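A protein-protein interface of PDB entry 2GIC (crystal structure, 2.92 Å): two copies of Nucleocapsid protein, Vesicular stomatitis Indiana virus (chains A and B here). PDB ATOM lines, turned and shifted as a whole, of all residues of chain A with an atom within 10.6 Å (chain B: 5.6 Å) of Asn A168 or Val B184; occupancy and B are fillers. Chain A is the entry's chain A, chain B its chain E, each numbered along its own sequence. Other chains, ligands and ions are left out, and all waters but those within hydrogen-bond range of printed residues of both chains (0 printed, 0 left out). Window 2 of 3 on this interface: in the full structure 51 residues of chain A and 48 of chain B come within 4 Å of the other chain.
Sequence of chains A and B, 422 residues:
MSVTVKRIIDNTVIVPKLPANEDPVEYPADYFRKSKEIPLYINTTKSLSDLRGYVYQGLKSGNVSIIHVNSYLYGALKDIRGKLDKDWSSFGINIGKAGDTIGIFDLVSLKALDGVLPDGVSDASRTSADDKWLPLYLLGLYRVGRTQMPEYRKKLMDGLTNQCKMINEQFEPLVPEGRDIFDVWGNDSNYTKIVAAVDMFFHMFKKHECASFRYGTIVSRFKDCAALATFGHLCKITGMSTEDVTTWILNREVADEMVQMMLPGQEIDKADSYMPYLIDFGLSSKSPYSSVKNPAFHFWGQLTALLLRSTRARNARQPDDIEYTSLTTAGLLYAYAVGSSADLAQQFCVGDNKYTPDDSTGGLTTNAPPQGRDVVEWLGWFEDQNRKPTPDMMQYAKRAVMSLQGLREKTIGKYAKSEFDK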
ATOM      1  N   ARG A 126      -4.040  28.120  40.147  1.00  0.00           N
ATOM      2  CA  ARG A 126      -3.726  27.666  38.792  1.00  0.00           C
ATOM      3  C   ARG A 126      -2.704  26.531  38.762  1.00  0.00           C
ATOM      4  O   ARG A 126      -1.605  26.650  39.309  1.00  0.00           O
ATOM      5  CB  ARG A 126      -3.282  28.835  37.902  1.00  0.00           C
ATOM      6  CG  ARG A 126      -4.431  29.532  37.178  1.00  0.00           C
ATOM      7  CD  ARG A 126      -4.987  28.664  36.052  1.00  0.00           C
ATOM      8  NE  ARG A 126      -6.408  28.916  35.807  1.00  0.00           N
ATOM      9  CZ  ARG A 126      -7.407  28.297  36.437  1.00  0.00           C
ATOM     10  NH1 ARG A 126      -7.159  27.379  37.363  1.00  0.00           N
ATOM     11  NH2 ARG A 126      -8.665  28.599  36.140  1.00  0.00           N
ATOM     12  N   ALA A 129      -1.132  24.118  33.891  1.00  0.00           N
ATOM     13  CA  ALA A 129      -1.624  24.535  32.585  1.00  0.00           C
ATOM     14  C   ALA A 129      -1.007  25.893  32.256  1.00  0.00           C
ATOM     15  O   ALA A 129      -1.661  26.765  31.683  1.00  0.00           O
ATOM     16  CB  ALA A 129      -3.142  24.613  32.584  1.00  0.00           C
ATOM     17  N   LYS A 132       1.143  25.669  28.608  1.00  0.00           N
ATOM     18  CA  LYS A 132       0.150  25.056  27.730  1.00  0.00           C
ATOM     19  C   LYS A 132      -0.758  26.054  27.003  1.00  0.00           C
ATOM     20  O   LYS A 132      -1.247  25.751  25.913  1.00  0.00           O
ATOM     21  CB  LYS A 132      -0.685  24.018  28.497  1.00  0.00           C
ATOM     22  CG  LYS A 132       0.068  22.729  28.844  1.00  0.00           C
ATOM     23  CD  LYS A 132       0.407  21.919  27.594  1.00  0.00           C
ATOM     24  CE  LYS A 132       1.454  20.855  27.879  1.00  0.00           C
ATOM     25  NZ  LYS A 132       2.016  20.306  26.615  1.00  0.00           N
ATOM     26  N   TRP A 133      -0.979  27.230  27.596  1.00  0.00           N
ATOM     27  CA  TRP A 133      -1.777  28.278  26.941  1.00  0.00           C
ATOM     28  C   TRP A 133      -1.422  29.719  27.305  1.00  0.00           C
ATOM     29  O   TRP A 133      -1.437  30.590  26.436  1.00  0.00           O
ATOM     30  CB  TRP A 133      -3.286  28.038  27.121  1.00  0.00           C
ATOM     31  CG  TRP A 133      -3.820  28.280  28.504  1.00  0.00           C
ATOM     32  CD1 TRP A 133      -3.753  27.430  29.568  1.00  0.00           C
ATOM     33  CD2 TRP A 133      -4.525  29.442  28.963  1.00  0.00           C
ATOM     34  NE1 TRP A 133      -4.361  27.991  30.665  1.00  0.00           N
ATOM     35  CE2 TRP A 133      -4.843  29.226  30.323  1.00  0.00           C
ATOM     36  CE3 TRP A 133      -4.913  30.646  28.360  1.00  0.00           C
ATOM     37  CZ2 TRP A 133      -5.532  30.170  31.092  1.00  0.00           C
ATOM     38  CZ3 TRP A 133      -5.599  31.585  29.125  1.00  0.00           C
ATOM     39  CH2 TRP A 133      -5.901  31.339  30.479  1.00  0.00           C
ATOM     40  N   LEU A 134      -1.098  29.965  28.574  1.00  0.00           N
ATOM     41  CA  LEU A 134      -0.901  31.333  29.084  1.00  0.00           C
ATOM     42  C   LEU A 134       0.152  32.178  28.338  1.00  0.00           C
ATOM     43  O   LEU A 134      -0.115  33.342  28.035  1.00  0.00           O
ATOM     44  CB  LEU A 134      -0.612  31.327  30.593  1.00  0.00           C
ATOM     45  CG  LEU A 134      -1.351  32.306  31.521  1.00  0.00           C
ATOM     46  CD1 LEU A 134      -0.662  32.352  32.878  1.00  0.00           C
ATOM     47  CD2 LEU A 134      -1.486  33.715  30.953  1.00  0.00           C
ATOM     48  N   LEU A 136       1.023  31.951  25.270  1.00  0.00           N
ATOM     49  CA  LEU A 136       0.402  32.257  23.982  1.00  0.00           C
ATOM     50  C   LEU A 136      -0.503  33.486  24.095  1.00  0.00           C
ATOM     51  O   LEU A 136      -0.417  34.406  23.280  1.00  0.00           O
ATOM     52  CB  LEU A 136      -0.395  31.046  23.478  1.00  0.00           C
ATOM     53  CG  LEU A 136      -0.645  30.828  21.980  1.00  0.00           C
ATOM     54  CD1 LEU A 136      -1.164  29.413  21.741  1.00  0.00           C
ATOM     55  CD2 LEU A 136      -1.602  31.858  21.383  1.00  0.00           C
ATOM     56  N   GLY A 159      -7.629  35.370  19.177  1.00  0.00           N
ATOM     57  CA  GLY A 159      -6.907  34.916  20.362  1.00  0.00           C
ATOM     58  C   GLY A 159      -7.571  33.720  21.022  1.00  0.00           C
ATOM     59  O   GLY A 159      -7.052  32.605  20.954  1.00  0.00           O
ATOM     60  N   LEU A 160      -8.736  33.951  21.632  1.00  0.00           N
ATOM     61  CA  LEU A 160      -9.413  32.933  22.444  1.00  0.00           C
ATOM     62  C   LEU A 160      -9.615  31.613  21.707  1.00  0.00           C
ATOM     63  O   LEU A 160      -9.574  30.549  22.322  1.00  0.00           O
ATOM     64  CB  LEU A 160     -10.753  33.448  23.001  1.00  0.00           C
ATOM     65  CG  LEU A 160     -12.066  32.988  22.348  1.00  0.00           C
ATOM     66  CD1 LEU A 160     -13.132  32.674  23.390  1.00  0.00           C
ATOM     67  CD2 LEU A 160     -12.572  33.994  21.327  1.00  0.00           C
ATOM     68  N   THR A 161      -9.830  31.692  20.397  1.00  0.00           N
ATOM     69  CA  THR A 161     -10.100  30.514  19.580  1.00  0.00           C
ATOM     70  C   THR A 161      -8.842  29.680  19.366  1.00  0.00           C
ATOM     71  O   THR A 161      -8.928  28.485  19.076  1.00  0.00           O
ATOM     72  CB  THR A 161     -10.707  30.897  18.220  1.00  0.00           C
ATOM     73  OG1 THR A 161      -9.923  31.937  17.624  1.00  0.00           O
ATOM     74  CG2 THR A 161     -12.138  31.385  18.391  1.00  0.00           C
ATOM     75  N   ASN A 162      -7.679  30.312  19.515  1.00  0.00           N
ATOM     76  CA  ASN A 162      -6.406  29.607  19.407  1.00  0.00           C
ATOM     77  C   ASN A 162      -5.967  28.958  20.723  1.00  0.00           C
ATOM     78  O   ASN A 162      -5.235  27.963  20.711  1.00  0.00           O
ATOM     79  CB  ASN A 162      -5.308  30.528  18.868  1.00  0.00           C
ATOM     80  CG  ASN A 162      -4.088  29.759  18.383  1.00  0.00           C
ATOM     81  OD1 ASN A 162      -4.204  28.798  17.621  1.00  0.00           O
ATOM     82  ND2 ASN A 162      -2.912  30.178  18.826  1.00  0.00           N
ATOM     83  N   GLN A 163      -6.411  29.526  21.845  1.00  0.00           N
ATOM     84  CA  GLN A 163      -6.164  28.945  23.172  1.00  0.00           C
ATOM     85  C   GLN A 163      -7.297  28.018  23.600  1.00  0.00           C
ATOM     86  O   GLN A 163      -7.165  27.275  24.573  1.00  0.00           O
ATOM     87  CB  GLN A 163      -5.965  30.025  24.240  1.00  0.00           C
ATOM     88  CG  GLN A 163      -4.851  31.015  23.959  1.00  0.00           C
ATOM     89  CD  GLN A 163      -5.368  32.321  23.403  1.00  0.00           C
ATOM     90  OE1 GLN A 163      -6.364  32.861  23.884  1.00  0.00           O
ATOM     91  NE2 GLN A 163      -4.691  32.844  22.385  1.00  0.00           N
ATOM     92  N   CYS A 164      -8.415  28.080  22.878  1.00  0.00           N
ATOM     93  CA  CYS A 164      -9.533  27.168  23.102  1.00  0.00           C
ATOM     94  C   CYS A 164      -9.331  25.884  22.297  1.00  0.00           C
ATOM     95  O   CYS A 164     -10.144  24.958  22.360  1.00  0.00           O
ATOM     96  CB  CYS A 164     -10.861  27.834  22.740  1.00  0.00           C
ATOM     97  SG  CYS A 164     -12.289  27.153  23.608  1.00  0.00           S
ATOM     98  N   LYS A 165      -8.238  25.849  21.538  1.00  0.00           N
ATOM     99  CA  LYS A 165      -7.815  24.654  20.825  1.00  0.00           C
ATOM    100  C   LYS A 165      -6.714  23.945  21.609  1.00  0.00           C
ATOM    101  O   LYS A 165      -5.675  24.539  21.923  1.00  0.00           O
ATOM    102  CB  LYS A 165      -7.341  24.999  19.407  1.00  0.00           C
ATOM    103  CG  LYS A 165      -8.464  25.345  18.439  1.00  0.00           C
ATOM    104  CD  LYS A 165      -7.923  25.626  17.043  1.00  0.00           C
ATOM    105  CE  LYS A 165      -8.992  26.220  16.129  1.00  0.00           C
ATOM    106  NZ  LYS A 165      -9.255  27.663  16.420  1.00  0.00           N
ATOM    107  N   MET A 166      -6.972  22.677  21.931  1.00  0.00           N
ATOM    108  CA  MET A 166      -6.045  21.798  22.665  1.00  0.00           C
ATOM    109  C   MET A 166      -5.972  22.115  24.166  1.00  0.00           C
ATOM    110  O   MET A 166      -5.228  21.470  24.912  1.00  0.00           O
ATOM    111  CB  MET A 166      -4.654  21.780  22.000  1.00  0.00           C
ATOM    112  CG  MET A 166      -4.661  21.186  20.585  1.00  0.00           C
ATOM    113  SD  MET A 166      -3.374  21.796  19.468  1.00  0.00           S
ATOM    114  CE  MET A 166      -4.038  23.387  18.976  1.00  0.00           C
ATOM    115  N   ILE A 167      -6.768  23.097  24.598  1.00  0.00           N
ATOM    116  CA  ILE A 167      -6.762  23.581  25.984  1.00  0.00           C
ATOM    117  C   ILE A 167      -8.184  23.878  26.506  1.00  0.00           C
ATOM    118  O   ILE A 167      -8.551  23.416  27.587  1.00  0.00           O
ATOM    119  CB  ILE A 167      -5.857  24.834  26.146  1.00  0.00           C
ATOM    120  CG1 ILE A 167      -4.554  24.680  25.346  1.00  0.00           C
ATOM    121  CG2 ILE A 167      -5.560  25.087  27.622  1.00  0.00           C
ATOM    122  CD1 ILE A 167      -4.236  25.845  24.430  1.00  0.00           C
ATOM    123  N   ASN A 168      -8.956  24.654  25.737  1.00  0.00           N
ATOM    124  CA  ASN A 168     -10.387  24.944  26.001  1.00  0.00           C
ATOM    125  C   ASN A 168     -10.681  25.942  27.137  1.00  0.00           C
ATOM    126  O   ASN A 168     -11.288  25.579  28.149  1.00  0.00           O
ATOM    127  CB  ASN A 168     -11.195  23.648  26.198  1.00  0.00           C
ATOM    128  CG  ASN A 168     -11.028  22.664  25.050  1.00  0.00           C
ATOM    129  OD1 ASN A 168     -11.592  22.849  23.968  1.00  0.00           O
ATOM    130  ND2 ASN A 168     -10.262  21.602  25.287  1.00  0.00           N
ATOM    131  N   GLU A 169     -10.277  27.200  26.952  1.00  0.00           N
ATOM    132  CA  GLU A 169     -10.427  28.233  27.995  1.00  0.00           C
ATOM    133  C   GLU A 169     -11.229  29.464  27.535  1.00  0.00           C
ATOM    134  O   GLU A 169     -11.826  29.449  26.456  1.00  0.00           O
ATOM    135  CB  GLU A 169      -9.055  28.651  28.543  1.00  0.00           C
ATOM    136  CG  GLU A 169      -8.146  27.488  28.977  1.00  0.00           C
ATOM    137  CD  GLU A 169      -8.790  26.543  29.992  1.00  0.00           C
ATOM    138  OE1 GLU A 169      -8.660  25.311  29.819  1.00  0.00           O
ATOM    139  OE2 GLU A 169      -9.421  27.022  30.960  1.00  0.00           O
ATOM    140  N   GLN A 170     -11.243  30.519  28.358  1.00  0.00           N
ATOM    141  CA  GLN A 170     -12.047  31.723  28.081  1.00  0.00           C
ATOM    142  C   GLN A 170     -11.258  33.041  28.208  1.00  0.00           C
ATOM    143  O   GLN A 170     -10.038  33.022  28.385  1.00  0.00           O
ATOM    144  CB  GLN A 170     -13.300  31.756  28.976  1.00  0.00           C
ATOM    145  CG  GLN A 170     -14.214  30.520  28.883  1.00  0.00           C
ATOM    146  CD  GLN A 170     -14.788  30.286  27.487  1.00  0.00           C
ATOM    147  OE1 GLN A 170     -15.422  31.167  26.904  1.00  0.00           O
ATOM    148  NE2 GLN A 170     -14.577  29.085  26.956  1.00  0.00           N
ATOM    149  N   PHE A 171     -11.968  34.171  28.107  1.00  0.00           N
ATOM    150  CA  PHE A 171     -11.391  35.526  28.222  1.00  0.00           C
ATOM    151  C   PHE A 171     -10.901  35.860  29.642  1.00  0.00           C
ATOM    152  O   PHE A 171     -11.171  35.112  30.585  1.00  0.00           O
ATOM    153  CB  PHE A 171     -12.425  36.587  27.815  1.00  0.00           C
ATOM    154  CG  PHE A 171     -12.880  36.506  26.380  1.00  0.00           C
ATOM    155  CD1 PHE A 171     -14.020  35.780  26.037  1.00  0.00           C
ATOM    156  CD2 PHE A 171     -12.195  37.192  25.377  1.00  0.00           C
ATOM    157  CE1 PHE A 171     -14.461  35.718  24.712  1.00  0.00           C
ATOM    158  CE2 PHE A 171     -12.625  37.136  24.047  1.00  0.00           C
ATOM    159  CZ  PHE A 171     -13.760  36.399  23.715  1.00  0.00           C
ATOM    160  N   GLU A 172     -10.198  36.988  29.788  1.00  0.00           N
ATOM    161  CA  GLU A 172      -9.745  37.469  31.108  1.00  0.00           C
ATOM    162  C   GLU A 172     -10.285  38.859  31.511  1.00  0.00           C
ATOM    163  O   GLU A 172     -11.234  38.928  32.294  1.00  0.00           O
ATOM    164  CB  GLU A 172      -8.219  37.371  31.259  1.00  0.00           C
ATOM    165  CG  GLU A 172      -7.726  36.095  31.935  1.00  0.00           C
ATOM    166  CD  GLU A 172      -8.010  34.837  31.129  1.00  0.00           C
ATOM    167  OE1 GLU A 172      -8.394  33.819  31.742  1.00  0.00           O
ATOM    168  OE2 GLU A 172      -7.854  34.863  29.888  1.00  0.00           O
ATOM    169  N   ASN B  63     -16.580  19.673  27.290  1.00  0.00           N
ATOM    170  CA  ASN B  63     -15.141  19.397  27.357  1.00  0.00           C
ATOM    171  C   ASN B  63     -14.782  17.913  27.194  1.00  0.00           C
ATOM    172  O   ASN B  63     -14.117  17.317  28.045  1.00  0.00           O
ATOM    173  CB  ASN B  63     -14.529  19.990  28.639  1.00  0.00           C
ATOM    174  CG  ASN B  63     -15.176  19.456  29.911  1.00  0.00           C
ATOM    175  OD1 ASN B  63     -16.324  19.007  29.908  1.00  0.00           O
ATOM    176  ND2 ASN B  63     -14.437  19.516  31.013  1.00  0.00           N
ATOM    177  N   ILE B  66     -10.288  14.479  23.219  1.00  0.00           N
ATOM    178  CA  ILE B  66      -9.997  13.975  21.882  1.00  0.00           C
ATOM    179  C   ILE B  66      -9.318  12.606  21.972  1.00  0.00           C
ATOM    180  O   ILE B  66      -9.539  11.737  21.130  1.00  0.00           O
ATOM    181  CB  ILE B  66      -9.171  14.994  21.033  1.00  0.00           C
ATOM    182  CG1 ILE B  66      -8.797  14.412  19.662  1.00  0.00           C
ATOM    183  CG2 ILE B  66      -7.925  15.478  21.789  1.00  0.00           C
ATOM    184  CD1 ILE B  66      -9.962  14.200  18.716  1.00  0.00           C
ATOM    185  N   ASP B 180     -14.523  26.846  17.847  1.00  0.00           N
ATOM    186  CA  ASP B 180     -14.365  26.917  19.303  1.00  0.00           C
ATOM    187  C   ASP B 180     -14.528  25.566  20.013  1.00  0.00           C
ATOM    188  O   ASP B 180     -13.800  25.267  20.963  1.00  0.00           O
ATOM    189  CB  ASP B 180     -15.365  27.930  19.879  1.00  0.00           C
ATOM    190  CG  ASP B 180     -14.707  28.961  20.783  1.00  0.00           C
ATOM    191  OD1 ASP B 180     -15.426  29.552  21.621  1.00  0.00           O
ATOM    192  OD2 ASP B 180     -13.484  29.192  20.651  1.00  0.00           O
ATOM    193  N   ILE B 181     -15.479  24.761  19.544  1.00  0.00           N
ATOM    194  CA  ILE B 181     -15.870  23.523  20.225  1.00  0.00           C
ATOM    195  C   ILE B 181     -15.046  22.304  19.775  1.00  0.00           C
ATOM    196  O   ILE B 181     -13.984  22.018  20.335  1.00  0.00           O
ATOM    197  CB  ILE B 181     -17.382  23.229  20.032  1.00  0.00           C
ATOM    198  CG1 ILE B 181     -18.181  24.530  19.888  1.00  0.00           C
ATOM    199  CG2 ILE B 181     -17.913  22.358  21.174  1.00  0.00           C
ATOM    200  CD1 ILE B 181     -19.447  24.384  19.064  1.00  0.00           C
ATOM    201  N   PHE B 182     -15.555  21.596  18.767  1.00  0.00           N
ATOM    202  CA  PHE B 182     -14.922  20.400  18.198  1.00  0.00           C
ATOM    203  C   PHE B 182     -13.767  20.735  17.250  1.00  0.00           C
ATOM    204  O   PHE B 182     -13.081  19.841  16.749  1.00  0.00           O
ATOM    205  CB  PHE B 182     -15.967  19.556  17.452  1.00  0.00           C
ATOM    206  CG  PHE B 182     -17.078  20.367  16.828  1.00  0.00           C
ATOM    207  CD1 PHE B 182     -16.804  21.354  15.878  1.00  0.00           C
ATOM    208  CD2 PHE B 182     -18.403  20.140  17.190  1.00  0.00           C
ATOM    209  CE1 PHE B 182     -17.830  22.106  15.311  1.00  0.00           C
ATOM    210  CE2 PHE B 182     -19.437  20.884  16.622  1.00  0.00           C
ATOM    211  CZ  PHE B 182     -19.150  21.868  15.681  1.00  0.00           C
ATOM    212  N   ASP B 183     -13.560  22.028  17.017  1.00  0.00           N
ATOM    213  CA  ASP B 183     -12.559  22.518  16.069  1.00  0.00           C
ATOM    214  C   ASP B 183     -11.127  22.291  16.555  1.00  0.00           C
ATOM    215  O   ASP B 183     -10.161  22.552  15.834  1.00  0.00           O
ATOM    216  CB  ASP B 183     -12.821  23.992  15.761  1.00  0.00           C
ATOM    217  CG  ASP B 183     -14.277  24.260  15.415  1.00  0.00           C
ATOM    218  OD1 ASP B 183     -14.566  24.559  14.236  1.00  0.00           O
ATOM    219  OD2 ASP B 183     -15.134  24.157  16.323  1.00  0.00           O
ATOM    220  N   VAL B 184     -11.012  21.802  17.787  1.00  0.00           N
ATOM    221  CA  VAL B 184      -9.761  21.312  18.350  1.00  0.00           C
ATOM    222  C   VAL B 184      -9.307  20.082  17.566  1.00  0.00           C
ATOM    223  O   VAL B 184      -8.113  19.903  17.301  1.00  0.00           O
ATOM    224  CB  VAL B 184      -9.952  20.899  19.836  1.00  0.00           C
ATOM    225  CG1 VAL B 184      -8.646  20.399  20.445  1.00  0.00           C
ATOM    226  CG2 VAL B 184     -10.546  22.045  20.653  1.00  0.00           C
ATOM    227  N   TRP B 185     -10.283  19.253  17.189  1.00  0.00           N
ATOM    228  CA  TRP B 185     -10.043  17.945  16.581  1.00  0.00           C
ATOM    229  C   TRP B 185      -9.303  18.008  15.244  1.00  0.00           C
ATOM    230  O   TRP B 185      -8.601  17.066  14.874  1.00  0.00           O
ATOM    231  CB  TRP B 185     -11.360  17.178  16.416  1.00  0.00           C
ATOM    232  CG  TRP B 185     -12.144  16.963  17.692  1.00  0.00           C
ATOM    233  CD1 TRP B 185     -11.694  17.111  18.975  1.00  0.00           C
ATOM    234  CD2 TRP B 185     -13.506  16.526  17.795  1.00  0.00           C
ATOM    235  NE1 TRP B 185     -12.695  16.809  19.867  1.00  0.00           N
ATOM    236  CE2 TRP B 185     -13.817  16.446  19.170  1.00  0.00           C
ATOM    237  CE3 TRP B 185     -14.495  16.200  16.859  1.00  0.00           C
ATOM    238  CZ2 TRP B 185     -15.076  16.055  19.633  1.00  0.00           C
ATOM    239  CZ3 TRP B 185     -15.748  15.808  17.320  1.00  0.00           C
ATOM    240  CH2 TRP B 185     -16.026  15.741  18.696  1.00  0.00           C
ATOM    241  N   GLY B 186      -9.471  19.116  14.526  1.00  0.00           N
ATOM    242  CA  GLY B 186      -8.706  19.372  13.310  1.00  0.00           C
ATOM    243  C   GLY B 186      -7.215  19.378  13.590  1.00  0.00           C
ATOM    244  O   GLY B 186      -6.450  18.691  12.914  1.00  0.00           O
ATOM    245  N   ASN B 187      -6.807  20.138  14.604  1.00  0.00           N
ATOM    246  CA  ASN B 187      -5.401  20.222  15.001  1.00  0.00           C
ATOM    247  C   ASN B 187      -4.866  18.987  15.739  1.00  0.00           C
ATOM    248  O   ASN B 187      -3.784  19.036  16.333  1.00  0.00           O
ATOM    249  CB  ASN B 187      -5.142  21.494  15.823  1.00  0.00           C
ATOM    250  CG  ASN B 187      -4.585  22.640  14.987  1.00  0.00           C
ATOM    251  OD1 ASN B 187      -4.734  23.808  15.347  1.00  0.00           O
ATOM    252  ND2 ASN B 187      -3.929  22.312  13.876  1.00  0.00           N
ATOM    253  N   ASP B 188      -5.617  17.888  15.697  1.00  0.00           N
ATOM    254  CA  ASP B 188      -5.153  16.623  16.259  1.00  0.00           C
ATOM    255  C   ASP B 188      -4.596  15.710  15.171  1.00  0.00           C
ATOM    256  O   ASP B 188      -5.296  15.353  14.221  1.00  0.00           O
ATOM    257  CB  ASP B 188      -6.263  15.923  17.047  1.00  0.00           C
ATOM    258  CG  ASP B 188      -5.760  14.704  17.810  1.00  0.00           C
ATOM    259  OD1 ASP B 188      -5.587  14.798  19.044  1.00  0.00           O
ATOM    260  OD2 ASP B 188      -5.525  13.655  17.171  1.00  0.00           O
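The side-chain sulfur (SG) of Cys A164 lies within hydrogen-bond range of the backbone carbonyl oxygen (O) of Asp B180, at 3.6 Å.
O of Gln A163 is in hydrogen-bond range of N of Asn A168 (3.4 Å). O of Glu A169 is in hydrogen-bond range of SG of Cys A164 (3.7 Å). The backbone carbonyl oxygen of Cys A164 sits close to the side-chain amide oxygen of Asn A168, at 3.0 Å. NZ of Lys A165 is in hydrogen-bond range of O of Thr A161 (2.8 Å). The backbone NH (N) of Asp B180 is in hydrogen-bond range of the side-chain carboxylate (OD2) of Asp B183 (3.2 Å). N of Ile B181 sits at hydrogen-bond distance from OD2 of Asp B183 (3.3 Å).
Among the printed residues, pairs that only touch across the chains: Met A166 with Val B184 (3.2 Å), Cys A164 with Val B184 (3.4 Å), Thr A161 with Asp B180 (3.4 Å), Asn A168 with Val B184 (3.6 Å), Met A166 with Asn B187 (3.7 Å), Lys A165 with Val B184 (3.8 Å) and Lys A165 with Asp B183 (3.9 Å).
Of the printed residues of chain B, Thr A161 touches Asp B180. Printed residues of chain B within 4 Å of Cys A164: Asp B180 and Val B184. Of the printed residues of chain B, Met A166 touches Val B184 (3.2 Å) and Asn B187 (3.7 Å). Of the printed residues of chain A, Asp B180 touches Thr A161 and Cys A164. Asp B183 touches just one residue of chain A: Lys A165. Of chain A, only Cys A164, Lys A165, Met A166 and Asn A168 come within 4 Å of Val B184. No residue of chain A comes within 4 Å of Gly B186. Asn B187 touches just one residue of chain A: Met A166 (3.7 Å). The nearest residue of chain A that does not touch Val B184 is Ile A167 (5.3 Å).
No position is printed for both chains. Of the 8 pairs that touch across the chains among the printed residues, none has its exchanged pair printed and touching as well.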
